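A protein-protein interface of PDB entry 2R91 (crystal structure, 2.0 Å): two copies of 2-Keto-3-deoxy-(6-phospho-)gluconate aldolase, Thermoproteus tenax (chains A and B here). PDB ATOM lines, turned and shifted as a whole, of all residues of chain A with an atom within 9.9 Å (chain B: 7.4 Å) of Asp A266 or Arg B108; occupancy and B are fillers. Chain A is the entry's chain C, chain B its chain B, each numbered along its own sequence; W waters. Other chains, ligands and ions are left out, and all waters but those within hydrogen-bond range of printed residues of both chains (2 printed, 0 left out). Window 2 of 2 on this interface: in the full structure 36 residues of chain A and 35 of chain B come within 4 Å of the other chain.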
ATOM      1  N   HIS A 236      24.182 -25.317  34.089  1.00  0.00           N
ATOM      2  CA  HIS A 236      25.492 -24.771  34.364  1.00  0.00           C
ATOM      3  C   HIS A 236      26.238 -24.415  33.090  1.00  0.00           C
ATOM      4  O   HIS A 236      26.982 -23.434  33.065  1.00  0.00           O
ATOM      5  CB  HIS A 236      26.295 -25.724  35.256  1.00  0.00           C
ATOM      6  CG  HIS A 236      27.696 -25.270  35.494  1.00  0.00           C
ATOM      7  ND1 HIS A 236      28.023 -24.365  36.482  1.00  0.00           N
ATOM      8  CD2 HIS A 236      28.852 -25.575  34.855  1.00  0.00           C
ATOM      9  CE1 HIS A 236      29.326 -24.138  36.445  1.00  0.00           C
ATOM     10  NE2 HIS A 236      29.853 -24.863  35.471  1.00  0.00           N
ATOM     11  N   ILE A 237      26.045 -25.162  32.009  1.00  0.00           N
ATOM     12  CA  ILE A 237      26.743 -24.800  30.779  1.00  0.00           C
ATOM     13  C   ILE A 237      25.897 -24.079  29.765  1.00  0.00           C
ATOM     14  O   ILE A 237      26.364 -23.815  28.665  1.00  0.00           O
ATOM     15  CB  ILE A 237      27.339 -26.031  30.042  1.00  0.00           C
ATOM     16  CG1 ILE A 237      26.260 -27.075  29.803  1.00  0.00           C
ATOM     17  CG2 ILE A 237      28.579 -26.595  30.791  1.00  0.00           C
ATOM     18  CD1 ILE A 237      26.658 -28.101  28.800  1.00  0.00           C
ATOM     19  N   GLY A 238      24.644 -23.785  30.085  1.00  0.00           N
ATOM     20  CA  GLY A 238      23.788 -23.137  29.092  1.00  0.00           C
ATOM     21  C   GLY A 238      22.713 -24.101  28.628  1.00  0.00           C
ATOM     22  O   GLY A 238      22.891 -24.821  27.633  1.00  0.00           O
ATOM     23  N   ALA A 241      21.235 -24.801  24.728  1.00  0.00           N
ATOM     24  CA  ALA A 241      22.091 -25.625  23.856  1.00  0.00           C
ATOM     25  C   ALA A 241      22.298 -27.024  24.426  1.00  0.00           C
ATOM     26  O   ALA A 241      22.403 -27.996  23.692  1.00  0.00           O
ATOM     27  CB  ALA A 241      23.413 -24.951  23.627  1.00  0.00           C
ATOM     28  N   ALA A 242      22.338 -27.129  25.744  1.00  0.00           N
ATOM     29  CA  ALA A 242      22.591 -28.401  26.406  1.00  0.00           C
ATOM     30  C   ALA A 242      21.495 -29.455  26.172  1.00  0.00           C
ATOM     31  O   ALA A 242      21.780 -30.654  26.136  1.00  0.00           O
ATOM     32  CB  ALA A 242      22.811 -28.176  27.912  1.00  0.00           C
ATOM     33  N   GLU A 245      22.461 -31.841  23.445  1.00  0.00           N
ATOM     34  CA  GLU A 245      23.457 -32.832  23.864  1.00  0.00           C
ATOM     35  C   GLU A 245      22.848 -33.901  24.774  1.00  0.00           C
ATOM     36  O   GLU A 245      23.138 -35.102  24.613  1.00  0.00           O
ATOM     37  CB  GLU A 245      24.654 -32.134  24.527  1.00  0.00           C
ATOM     38  CG  GLU A 245      25.833 -33.063  24.856  1.00  0.00           C
ATOM     39  CD  GLU A 245      26.452 -33.747  23.634  1.00  0.00           C
ATOM     40  OE1 GLU A 245      26.236 -33.313  22.489  1.00  0.00           O
ATOM     41  OE2 GLU A 245      27.172 -34.747  23.818  1.00  0.00           O
ATOM     42  N   GLU A 257      21.535 -29.223  16.008  1.00  0.00           N
ATOM     43  CA  GLU A 257      22.033 -28.167  16.884  1.00  0.00           C
ATOM     44  C   GLU A 257      21.116 -26.954  16.868  1.00  0.00           C
ATOM     45  O   GLU A 257      20.196 -26.892  16.045  1.00  0.00           O
ATOM     46  CB  GLU A 257      23.459 -27.788  16.492  1.00  0.00           C
ATOM     47  CG  GLU A 257      23.630 -27.586  15.023  1.00  0.00           C
ATOM     48  CD  GLU A 257      25.084 -27.371  14.615  1.00  0.00           C
ATOM     49  OE1 GLU A 257      25.995 -27.839  15.347  1.00  0.00           O
ATOM     50  OE2 GLU A 257      25.307 -26.735  13.549  1.00  0.00           O
ATOM     51  N   PRO A 258      21.304 -26.031  17.843  1.00  0.00           N
ATOM     52  CA  PRO A 258      20.580 -24.749  17.837  1.00  0.00           C
ATOM     53  C   PRO A 258      21.235 -23.766  16.874  1.00  0.00           C
ATOM     54  O   PRO A 258      22.153 -24.130  16.167  1.00  0.00           O
ATOM     55  CB  PRO A 258      20.673 -24.267  19.286  1.00  0.00           C
ATOM     56  CG  PRO A 258      21.871 -25.002  19.899  1.00  0.00           C
ATOM     57  CD  PRO A 258      22.160 -26.215  19.029  1.00  0.00           C
ATOM     58  N   GLY A 260      22.820 -19.715  16.442  1.00  0.00           N
ATOM     59  CA  GLY A 260      23.209 -18.545  17.179  1.00  0.00           C
ATOM     60  C   GLY A 260      22.338 -17.297  17.118  1.00  0.00           C
ATOM     61  O   GLY A 260      21.655 -17.059  16.089  1.00  0.00           O
ATOM     62  N   PRO A 261      22.014 -16.791  18.303  1.00  0.00           N
ATOM     63  CA  PRO A 261      22.849 -16.443  19.450  1.00  0.00           C
ATOM     64  C   PRO A 261      22.771 -17.654  20.392  1.00  0.00           C
ATOM     65  O   PRO A 261      23.511 -17.748  21.391  1.00  0.00           O
ATOM     66  CB  PRO A 261      22.158 -15.220  20.068  1.00  0.00           C
ATOM     67  CG  PRO A 261      20.740 -15.253  19.558  1.00  0.00           C
ATOM     68  CD  PRO A 261      20.751 -16.016  18.268  1.00  0.00           C
ATOM     69  N   VAL A 262      21.871 -18.604  20.105  1.00  0.00           N
ATOM     70  CA  VAL A 262      21.901 -19.854  20.854  1.00  0.00           C
ATOM     71  C   VAL A 262      22.893 -20.823  20.207  1.00  0.00           C
ATOM     72  O   VAL A 262      22.500 -21.799  19.558  1.00  0.00           O
ATOM     73  CB  VAL A 262      20.511 -20.493  21.012  1.00  0.00           C
ATOM     74  CG1 VAL A 262      20.536 -21.596  22.053  1.00  0.00           C
ATOM     75  CG2 VAL A 262      19.475 -19.419  21.373  1.00  0.00           C
ATOM     76  N   TYR A 263      24.189 -20.549  20.393  1.00  0.00           N
ATOM     77  CA  TYR A 263      25.247 -21.351  19.763  1.00  0.00           C
ATOM     78  C   TYR A 263      25.327 -22.742  20.337  1.00  0.00           C
ATOM     79  O   TYR A 263      25.196 -22.948  21.543  1.00  0.00           O
ATOM     80  CB  TYR A 263      26.631 -20.644  19.852  1.00  0.00           C
ATOM     81  CG  TYR A 263      26.618 -19.265  19.220  1.00  0.00           C
ATOM     82  CD1 TYR A 263      26.753 -19.107  17.862  1.00  0.00           C
ATOM     83  CD2 TYR A 263      26.421 -18.125  19.996  1.00  0.00           C
ATOM     84  CE1 TYR A 263      26.705 -17.844  17.273  1.00  0.00           C
ATOM     85  CE2 TYR A 263      26.381 -16.856  19.423  1.00  0.00           C
ATOM     86  CZ  TYR A 263      26.530 -16.720  18.070  1.00  0.00           C
ATOM     87  OH  TYR A 263      26.469 -15.470  17.479  1.00  0.00           O
ATOM     88  N   PRO A 264      25.542 -23.727  19.462  1.00  0.00           N
ATOM     89  CA  PRO A 264      25.740 -25.108  19.893  1.00  0.00           C
ATOM     90  C   PRO A 264      26.847 -25.208  20.959  1.00  0.00           C
ATOM     91  O   PRO A 264      27.701 -24.315  21.046  1.00  0.00           O
ATOM     92  CB  PRO A 264      26.119 -25.806  18.591  1.00  0.00           C
ATOM     93  CG  PRO A 264      25.445 -24.997  17.522  1.00  0.00           C
ATOM     94  CD  PRO A 264      25.606 -23.583  17.991  1.00  0.00           C
ATOM     95  N   LEU A 265      26.792 -26.227  21.815  1.00  0.00           N
ATOM     96  CA  LEU A 265      27.862 -26.454  22.783  1.00  0.00           C
ATOM     97  C   LEU A 265      29.172 -26.716  22.031  1.00  0.00           C
ATOM     98  O   LEU A 265      29.149 -27.161  20.877  1.00  0.00           O
ATOM     99  CB  LEU A 265      27.538 -27.619  23.736  1.00  0.00           C
ATOM    100  CG  LEU A 265      26.386 -27.527  24.744  1.00  0.00           C
ATOM    101  CD1 LEU A 265      26.396 -28.772  25.625  1.00  0.00           C
ATOM    102  CD2 LEU A 265      26.434 -26.240  25.617  1.00  0.00           C
ATOM    103  N   ASP A 266      30.307 -26.365  22.646  1.00  0.00           N
ATOM    104  CA  ASP A 266      31.607 -26.686  22.039  1.00  0.00           C
ATOM    105  C   ASP A 266      32.070 -28.062  22.553  1.00  0.00           C
ATOM    106  O   ASP A 266      31.524 -28.572  23.549  1.00  0.00           O
ATOM    107  CB  ASP A 266      32.657 -25.553  22.217  1.00  0.00           C
ATOM    108  CG  ASP A 266      33.067 -25.295  23.671  1.00  0.00           C
ATOM    109  OD1 ASP A 266      32.938 -26.183  24.549  1.00  0.00           O
ATOM    110  OD2 ASP A 266      33.576 -24.171  23.957  1.00  0.00           O
ATOM    111  N   PRO A 267      33.044 -28.697  21.850  1.00  0.00           N
ATOM    112  CA  PRO A 267      33.540 -30.026  22.244  1.00  0.00           C
ATOM    113  C   PRO A 267      33.861 -30.146  23.732  1.00  0.00           C
ATOM    114  O   PRO A 267      33.562 -31.172  24.358  1.00  0.00           O
ATOM    115  CB  PRO A 267      34.811 -30.177  21.393  1.00  0.00           C
ATOM    116  CG  PRO A 267      34.465 -29.442  20.131  1.00  0.00           C
ATOM    117  CD  PRO A 267      33.707 -28.214  20.616  1.00  0.00           C
ATOM    118  N   GLU A 268      34.431 -29.100  24.310  1.00  0.00           N
ATOM    119  CA  GLU A 268      34.747 -29.094  25.742  1.00  0.00           C
ATOM    120  C   GLU A 268      33.513 -29.115  26.650  1.00  0.00           C
ATOM    121  O   GLU A 268      33.494 -29.777  27.705  1.00  0.00           O
ATOM    122  CB  GLU A 268      35.597 -27.861  26.053  1.00  0.00           C
ATOM    123  CG  GLU A 268      35.944 -27.679  27.512  1.00  0.00           C
ATOM    124  CD  GLU A 268      37.037 -26.621  27.705  1.00  0.00           C
ATOM    125  OE1 GLU A 268      37.430 -25.973  26.693  1.00  0.00           O
ATOM    126  OE2 GLU A 268      37.505 -26.439  28.860  1.00  0.00           O
ATOM    127  N   GLU A 269      32.485 -28.364  26.259  1.00  0.00           N
ATOM    128  CA  GLU A 269      31.264 -28.277  27.062  1.00  0.00           C
ATOM    129  C   GLU A 269      30.537 -29.599  27.032  1.00  0.00           C
ATOM    130  O   GLU A 269      30.003 -30.043  28.048  1.00  0.00           O
ATOM    131  CB  GLU A 269      30.370 -27.137  26.555  1.00  0.00           C
ATOM    132  CG  GLU A 269      30.855 -25.760  27.034  1.00  0.00           C
ATOM    133  CD  GLU A 269      30.290 -24.608  26.215  1.00  0.00           C
ATOM    134  OE1 GLU A 269      30.031 -24.804  25.002  1.00  0.00           O
ATOM    135  OE2 GLU A 269      30.121 -23.492  26.781  1.00  0.00           O
ATOM    136  N   LYS A 270      30.523 -30.222  25.862  1.00  0.00           N
ATOM    137  CA  LYS A 270      29.910 -31.537  25.700  1.00  0.00           C
ATOM    138  C   LYS A 270      30.592 -32.590  26.553  1.00  0.00           C
ATOM    139  O   LYS A 270      29.923 -33.399  27.191  1.00  0.00           O
ATOM    140  CB  LYS A 270      29.971 -31.962  24.246  1.00  0.00           C
ATOM    141  CG  LYS A 270      29.280 -30.993  23.301  1.00  0.00           C
ATOM    142  CD  LYS A 270      29.173 -31.587  21.914  1.00  0.00           C
ATOM    143  CE  LYS A 270      28.454 -30.636  20.999  1.00  0.00           C
ATOM    144  NZ  LYS A 270      28.440 -31.178  19.606  1.00  0.00           N
ATOM    145  N   ALA A 271      31.929 -32.592  26.559  1.00  0.00           N
ATOM    146  CA  ALA A 271      32.671 -33.547  27.374  1.00  0.00           C
ATOM    147  C   ALA A 271      32.351 -33.323  28.831  1.00  0.00           C
ATOM    148  O   ALA A 271      32.125 -34.280  29.577  1.00  0.00           O
ATOM    149  CB  ALA A 271      34.208 -33.420  27.124  1.00  0.00           C
ATOM    150  N   TRP A 272      32.329 -32.058  29.256  1.00  0.00           N
ATOM    151  CA  TRP A 272      31.981 -31.746  30.637  1.00  0.00           C
ATOM    152  C   TRP A 272      30.582 -32.233  31.001  1.00  0.00           C
ATOM    153  O   TRP A 272      30.355 -32.768  32.094  1.00  0.00           O
ATOM    154  CB  TRP A 272      32.086 -30.241  30.897  1.00  0.00           C
ATOM    155  CG  TRP A 272      31.784 -29.909  32.316  1.00  0.00           C
ATOM    156  CD1 TRP A 272      32.681 -29.840  33.342  1.00  0.00           C
ATOM    157  CD2 TRP A 272      30.489 -29.624  32.892  1.00  0.00           C
ATOM    158  NE1 TRP A 272      32.029 -29.538  34.520  1.00  0.00           N
ATOM    159  CE2 TRP A 272      30.688 -29.397  34.270  1.00  0.00           C
ATOM    160  CE3 TRP A 272      29.180 -29.553  32.373  1.00  0.00           C
ATOM    161  CZ2 TRP A 272      29.636 -29.096  35.141  1.00  0.00           C
ATOM    162  CZ3 TRP A 272      28.142 -29.259  33.231  1.00  0.00           C
ATOM    163  CH2 TRP A 272      28.370 -29.035  34.603  1.00  0.00           C
ATOM    164  N   LEU A 273      29.615 -32.028  30.106  1.00  0.00           N
ATOM    165  CA  LEU A 273      28.239 -32.450  30.419  1.00  0.00           C
ATOM    166  C   LEU A 273      28.135 -33.969  30.555  1.00  0.00           C
ATOM    167  O   LEU A 273      27.483 -34.484  31.467  1.00  0.00           O
ATOM    168  CB  LEU A 273      27.286 -31.961  29.320  1.00  0.00           C
ATOM    169  CG  LEU A 273      25.781 -32.112  29.588  1.00  0.00           C
ATOM    170  CD1 LEU A 273      25.378 -31.432  30.901  1.00  0.00           C
ATOM    171  CD2 LEU A 273      24.998 -31.575  28.401  1.00  0.00           C
ATOM    172  N   ARG A 274      28.778 -34.696  29.648  1.00  0.00           N
ATOM    173  CA  ARG A 274      28.697 -36.159  29.674  1.00  0.00           C
ATOM    174  C   ARG A 274      29.192 -36.717  31.002  1.00  0.00           C
ATOM    175  O   ARG A 274      28.547 -37.581  31.608  1.00  0.00           O
ATOM    176  CB  ARG A 274      29.495 -36.762  28.522  1.00  0.00           C
ATOM    177  CG  ARG A 274      29.018 -36.309  27.149  1.00  0.00           C
ATOM    178  CD  ARG A 274      29.754 -37.032  26.026  1.00  0.00           C
ATOM    179  NE  ARG A 274      29.418 -36.507  24.693  1.00  0.00           N
ATOM    180  CZ  ARG A 274      30.293 -35.945  23.851  1.00  0.00           C
ATOM    181  NH1 ARG A 274      31.581 -35.831  24.196  1.00  0.00           N
ATOM    182  NH2 ARG A 274      29.878 -35.515  22.647  1.00  0.00           N
ATOM    183  N   LEU B 105      21.054 -18.623  28.719  1.00  0.00           N
ATOM    184  CA  LEU B 105      22.161 -18.433  27.784  1.00  0.00           C
ATOM    185  C   LEU B 105      23.442 -18.288  28.570  1.00  0.00           C
ATOM    186  O   LEU B 105      23.427 -17.776  29.695  1.00  0.00           O
ATOM    187  CB  LEU B 105      21.966 -17.247  26.832  1.00  0.00           C
ATOM    188  CG  LEU B 105      20.806 -17.216  25.793  1.00  0.00           C
ATOM    189  CD1 LEU B 105      21.006 -16.088  24.838  1.00  0.00           C
ATOM    190  CD2 LEU B 105      20.596 -18.532  25.003  1.00  0.00           C
ATOM    191  N   SER B 106      24.541 -18.786  27.999  1.00  0.00           N
ATOM    192  CA  SER B 106      25.816 -18.829  28.708  1.00  0.00           C
ATOM    193  C   SER B 106      26.635 -17.581  28.396  1.00  0.00           C
ATOM    194  O   SER B 106      26.443 -16.951  27.368  1.00  0.00           O
ATOM    195  CB  SER B 106      26.611 -20.068  28.291  1.00  0.00           C
ATOM    196  OG  SER B 106      27.068 -19.895  26.960  1.00  0.00           O
ATOM    197  N   GLU B 107      27.588 -17.243  29.268  1.00  0.00           N
ATOM    198  CA  GLU B 107      28.510 -16.130  28.983  1.00  0.00           C
ATOM    199  C   GLU B 107      29.234 -16.313  27.652  1.00  0.00           C
ATOM    200  O   GLU B 107      29.463 -15.348  26.910  1.00  0.00           O
ATOM    201  CB  GLU B 107      29.530 -15.974  30.125  1.00  0.00           C
ATOM    202  CG  GLU B 107      28.945 -15.310  31.348  1.00  0.00           C
ATOM    203  CD  GLU B 107      29.936 -15.218  32.515  1.00  0.00           C
ATOM    204  OE1 GLU B 107      31.170 -15.153  32.260  1.00  0.00           O
ATOM    205  OE2 GLU B 107      29.475 -15.208  33.694  1.00  0.00           O
ATOM    206  N   ARG B 108      29.584 -17.556  27.338  1.00  0.00           N
ATOM    207  CA  ARG B 108      30.258 -17.863  26.098  1.00  0.00           C
ATOM    208  C   ARG B 108      29.410 -17.555  24.871  1.00  0.00           C
ATOM    209  O   ARG B 108      29.918 -17.071  23.853  1.00  0.00           O
ATOM    210  CB  ARG B 108      30.690 -19.342  26.086  1.00  0.00           C
ATOM    211  CG  ARG B 108      31.495 -19.709  24.857  1.00  0.00           C
ATOM    212  CD  ARG B 108      31.848 -21.221  24.785  1.00  0.00           C
ATOM    213  NE  ARG B 108      30.764 -22.050  24.237  1.00  0.00           N
ATOM    214  CZ  ARG B 108      30.433 -22.094  22.947  1.00  0.00           C
ATOM    215  NH1 ARG B 108      31.089 -21.355  22.061  1.00  0.00           N
ATOM    216  NH2 ARG B 108      29.427 -22.870  22.546  1.00  0.00           N
ATOM    217  N   GLN B 109      28.111 -17.859  24.937  1.00  0.00           N
ATOM    218  CA  GLN B 109      27.231 -17.554  23.805  1.00  0.00           C
ATOM    219  C   GLN B 109      27.097 -16.049  23.613  1.00  0.00           C
ATOM    220  O   GLN B 109      27.110 -15.558  22.503  1.00  0.00           O
ATOM    221  CB  GLN B 109      25.850 -18.177  24.040  1.00  0.00           C
ATOM    222  CG  GLN B 109      25.828 -19.715  23.874  1.00  0.00           C
ATOM    223  CD  GLN B 109      24.520 -20.338  24.361  1.00  0.00           C
ATOM    224  OE1 GLN B 109      23.911 -19.858  25.328  1.00  0.00           O
ATOM    225  NE2 GLN B 109      24.082 -21.427  23.703  1.00  0.00           N
ATOM    226  N   ILE B 110      26.951 -15.315  24.707  1.00  0.00           N
ATOM    227  CA  ILE B 110      26.861 -13.862  24.613  1.00  0.00           C
ATOM    228  C   ILE B 110      28.146 -13.235  24.054  1.00  0.00           C
ATOM    229  O   ILE B 110      28.102 -12.403  23.148  1.00  0.00           O
ATOM    230  CB  ILE B 110      26.418 -13.222  25.951  1.00  0.00           C
ATOM    231  CG1 ILE B 110      24.994 -13.709  26.277  1.00  0.00           C
ATOM    232  CG2 ILE B 110      26.398 -11.682  25.802  1.00  0.00           C
ATOM    233  CD1 ILE B 110      24.744 -13.908  27.735  1.00  0.00           C
ATOM    234  N   ALA B 111      29.295 -13.673  24.553  1.00  0.00           N
ATOM    235  CA  ALA B 111      30.581 -13.145  24.029  1.00  0.00           C
ATOM    236  C   ALA B 111      30.772 -13.458  22.547  1.00  0.00           C
ATOM    237  O   ALA B 111      31.149 -12.581  21.758  1.00  0.00           O
ATOM    238  CB  ALA B 111      31.738 -13.695  24.839  1.00  0.00           C
ATOM    239  N   LYS B 112      30.508 -14.710  22.155  1.00  0.00           N
ATOM    240  CA  LYS B 112      30.593 -15.084  20.748  1.00  0.00           C
ATOM    241  C   LYS B 112      29.722 -14.199  19.861  1.00  0.00           C
ATOM    242  O   LYS B 112      30.141 -13.778  18.780  1.00  0.00           O
ATOM    243  CB  LYS B 112      30.242 -16.573  20.532  1.00  0.00           C
ATOM    244  CG  LYS B 112      30.182 -16.951  19.054  1.00  0.00           C
ATOM    245  CD  LYS B 112      30.430 -18.429  18.865  1.00  0.00           C
ATOM    246  CE  LYS B 112      30.249 -18.910  17.431  1.00  0.00           C
ATOM    247  NZ  LYS B 112      30.736 -18.026  16.329  1.00  0.00           N
ATOM    248  N   TYR B 113      28.507 -13.884  20.308  1.00  0.00           N
ATOM    249  CA  TYR B 113      27.635 -13.014  19.502  1.00  0.00           C
ATOM    250  C   TYR B 113      28.240 -11.629  19.280  1.00  0.00           C
ATOM    251  O   TYR B 113      28.254 -11.093  18.152  1.00  0.00           O
ATOM    252  CB  TYR B 113      26.257 -12.876  20.186  1.00  0.00           C
ATOM    253  CG  TYR B 113      25.355 -11.881  19.501  1.00  0.00           C
ATOM    254  CD1 TYR B 113      24.615 -12.245  18.387  1.00  0.00           C
ATOM    255  CD2 TYR B 113      25.215 -10.587  20.005  1.00  0.00           C
ATOM    256  CE1 TYR B 113      23.781 -11.338  17.752  1.00  0.00           C
ATOM    257  CE2 TYR B 113      24.389  -9.677  19.398  1.00  0.00           C
ATOM    258  CZ  TYR B 113      23.666 -10.053  18.271  1.00  0.00           C
ATOM    259  OH  TYR B 113      22.860  -9.134  17.652  1.00  0.00           O
ATOM    260  N   PHE B 114      28.750 -11.016  20.350  1.00  0.00           N
ATOM    261  CA  PHE B 114      29.335  -9.677  20.143  1.00  0.00           C
ATOM    262  C   PHE B 114      30.663  -9.709  19.356  1.00  0.00           C
ATOM    263  O   PHE B 114      30.939  -8.826  18.536  1.00  0.00           O
ATOM    264  CB  PHE B 114      29.485  -8.929  21.457  1.00  0.00           C
ATOM    265  CG  PHE B 114      28.184  -8.330  21.947  1.00  0.00           C
ATOM    266  CD1 PHE B 114      27.682  -7.162  21.376  1.00  0.00           C
ATOM    267  CD2 PHE B 114      27.470  -8.952  22.954  1.00  0.00           C
ATOM    268  CE1 PHE B 114      26.480  -6.612  21.805  1.00  0.00           C
ATOM    269  CE2 PHE B 114      26.248  -8.417  23.394  1.00  0.00           C
ATOM    270  CZ  PHE B 114      25.773  -7.268  22.825  1.00  0.00           C
ATOM    271  N   ARG B 115      31.477 -10.730  19.598  1.00  0.00           N
ATOM    272  CA  ARG B 115      32.773 -10.806  18.897  1.00  0.00           C
ATOM    273  C   ARG B 115      32.570 -11.063  17.399  1.00  0.00           C
ATOM    274  O   ARG B 115      33.230 -10.431  16.567  1.00  0.00           O
ATOM    275  CB  ARG B 115      33.715 -11.810  19.582  1.00  0.00           C
ATOM    276  CG  ARG B 115      34.233 -11.279  20.947  1.00  0.00           C
ATOM    277  CD  ARG B 115      34.799 -12.388  21.836  1.00  0.00           C
ATOM    278  NE  ARG B 115      35.184 -11.879  23.161  1.00  0.00           N
ATOM    279  CZ  ARG B 115      35.581 -12.642  24.176  1.00  0.00           C
ATOM    280  NH1 ARG B 115      35.653 -13.961  24.015  1.00  0.00           N
ATOM    281  NH2 ARG B 115      35.901 -12.104  25.353  1.00  0.00           N
HETATM  282  O   HOH W   1      27.696 -22.189  25.996  1.00  0.00           O
HETATM  283  O   HOH W   2      22.295 -22.251  25.975  1.00  0.00           O
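O of Pro A264 is in hydrogen-bond range of NH2 of Arg B108, 2.7 Å away.
The side-chain carboxylate of Glu A269 is in salt-bridge range of the guanidinium group of Arg B108 (3.0 Å).
The guanidinium group (NE) of Arg B108 lies within salt-bridge range of the side-chain carboxylate (OD2) of Asp A266, at 3.5 Å.
O of Tyr A263 lies within hydrogen-bond range of NE2 of Gln B109.
The side-chain hydroxyl (OG) of Ser B106 lies close to the backbone NH (N) of Arg B108 (3.5 Å).
N of Glu A268 lies close to OD1 of Asp A266.
The side-chain carboxylate (OD1) of Asp A266 lies within hydrogen-bond range of the backbone NH (N) of Glu A269 (2.8 Å).
The backbone NH (N) of Ser B106 is in hydrogen-bond range of the side-chain amide oxygen (OE1) of Gln B109 (2.9 Å).
Among the printed residues, merely in contact across the chains: Tyr A263 with Tyr B113, Tyr A263 with Lys B112, Pro A261 with Gln B109, Ala A241 with Gln B109, Val A262 with Gln B109, Ile A237 with Ser B106, Leu A265 with Arg B108 and Val A262 with Leu B105.
Of the printed residues of chain B, Ile A237 touches Ser B106 (3.8 Å).
Of the printed residues of chain B, Pro A261 touches Gln B109.
Of the printed residues of chain B, Pro A264 touches Arg B108.
Of the printed residues of chain B, Leu A265 touches Arg B108 (3.9 Å).
Of chain B, only Arg B108 comes within 4 Å of Asp A266.
Arg B108 touches just these residues of chain A: Pro A264, Leu A265, Asp A266 and Glu A269.
Ala B111 touches none of the printed residues of chain A.
The nearest printed residue of chain B that does not touch Asp A266 is Gln B109 (8.0 Å).
The nearest residue of chain A that does not touch Arg B108 is Tyr A263 (4.3 Å).
The nearest printed residue of chain A that does not touch Lys B112 is Pro A264 (6.6 Å).
Hydrophobic or aromatic side chains of chain A that line the printed part of chain B: Ala A241, Val A262 and Tyr A263.
Hydrophobic or aromatic side chains of chain B within 4 Å of the printed part of chain A: Leu B105 and Tyr B113.
Along chain B the printed residues that touch a printed residue of chain A span positions 105 to 113.
Among the printed residues, Asp or Glu carboxylates within 4 Å of a Lys or Arg side-chain nitrogen of the other chain: Asp A266 with Arg B108 and Glu A269 with Arg B108.
No position is printed for both chains.
Of the 12 pairs that touch across the chains among the printed residues, none has its exchanged pair printed and touching as well.
Water W1 lies within hydrogen-bond range of OG of Ser B106, OE2 of Glu A269 and O of Ile A237.
Water W2 lies within hydrogen-bond range of OE1 of Gln B109 (3.0 Å), N of Ala A241 (3.0 Å) and O of Gly A238 (3.1 Å).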
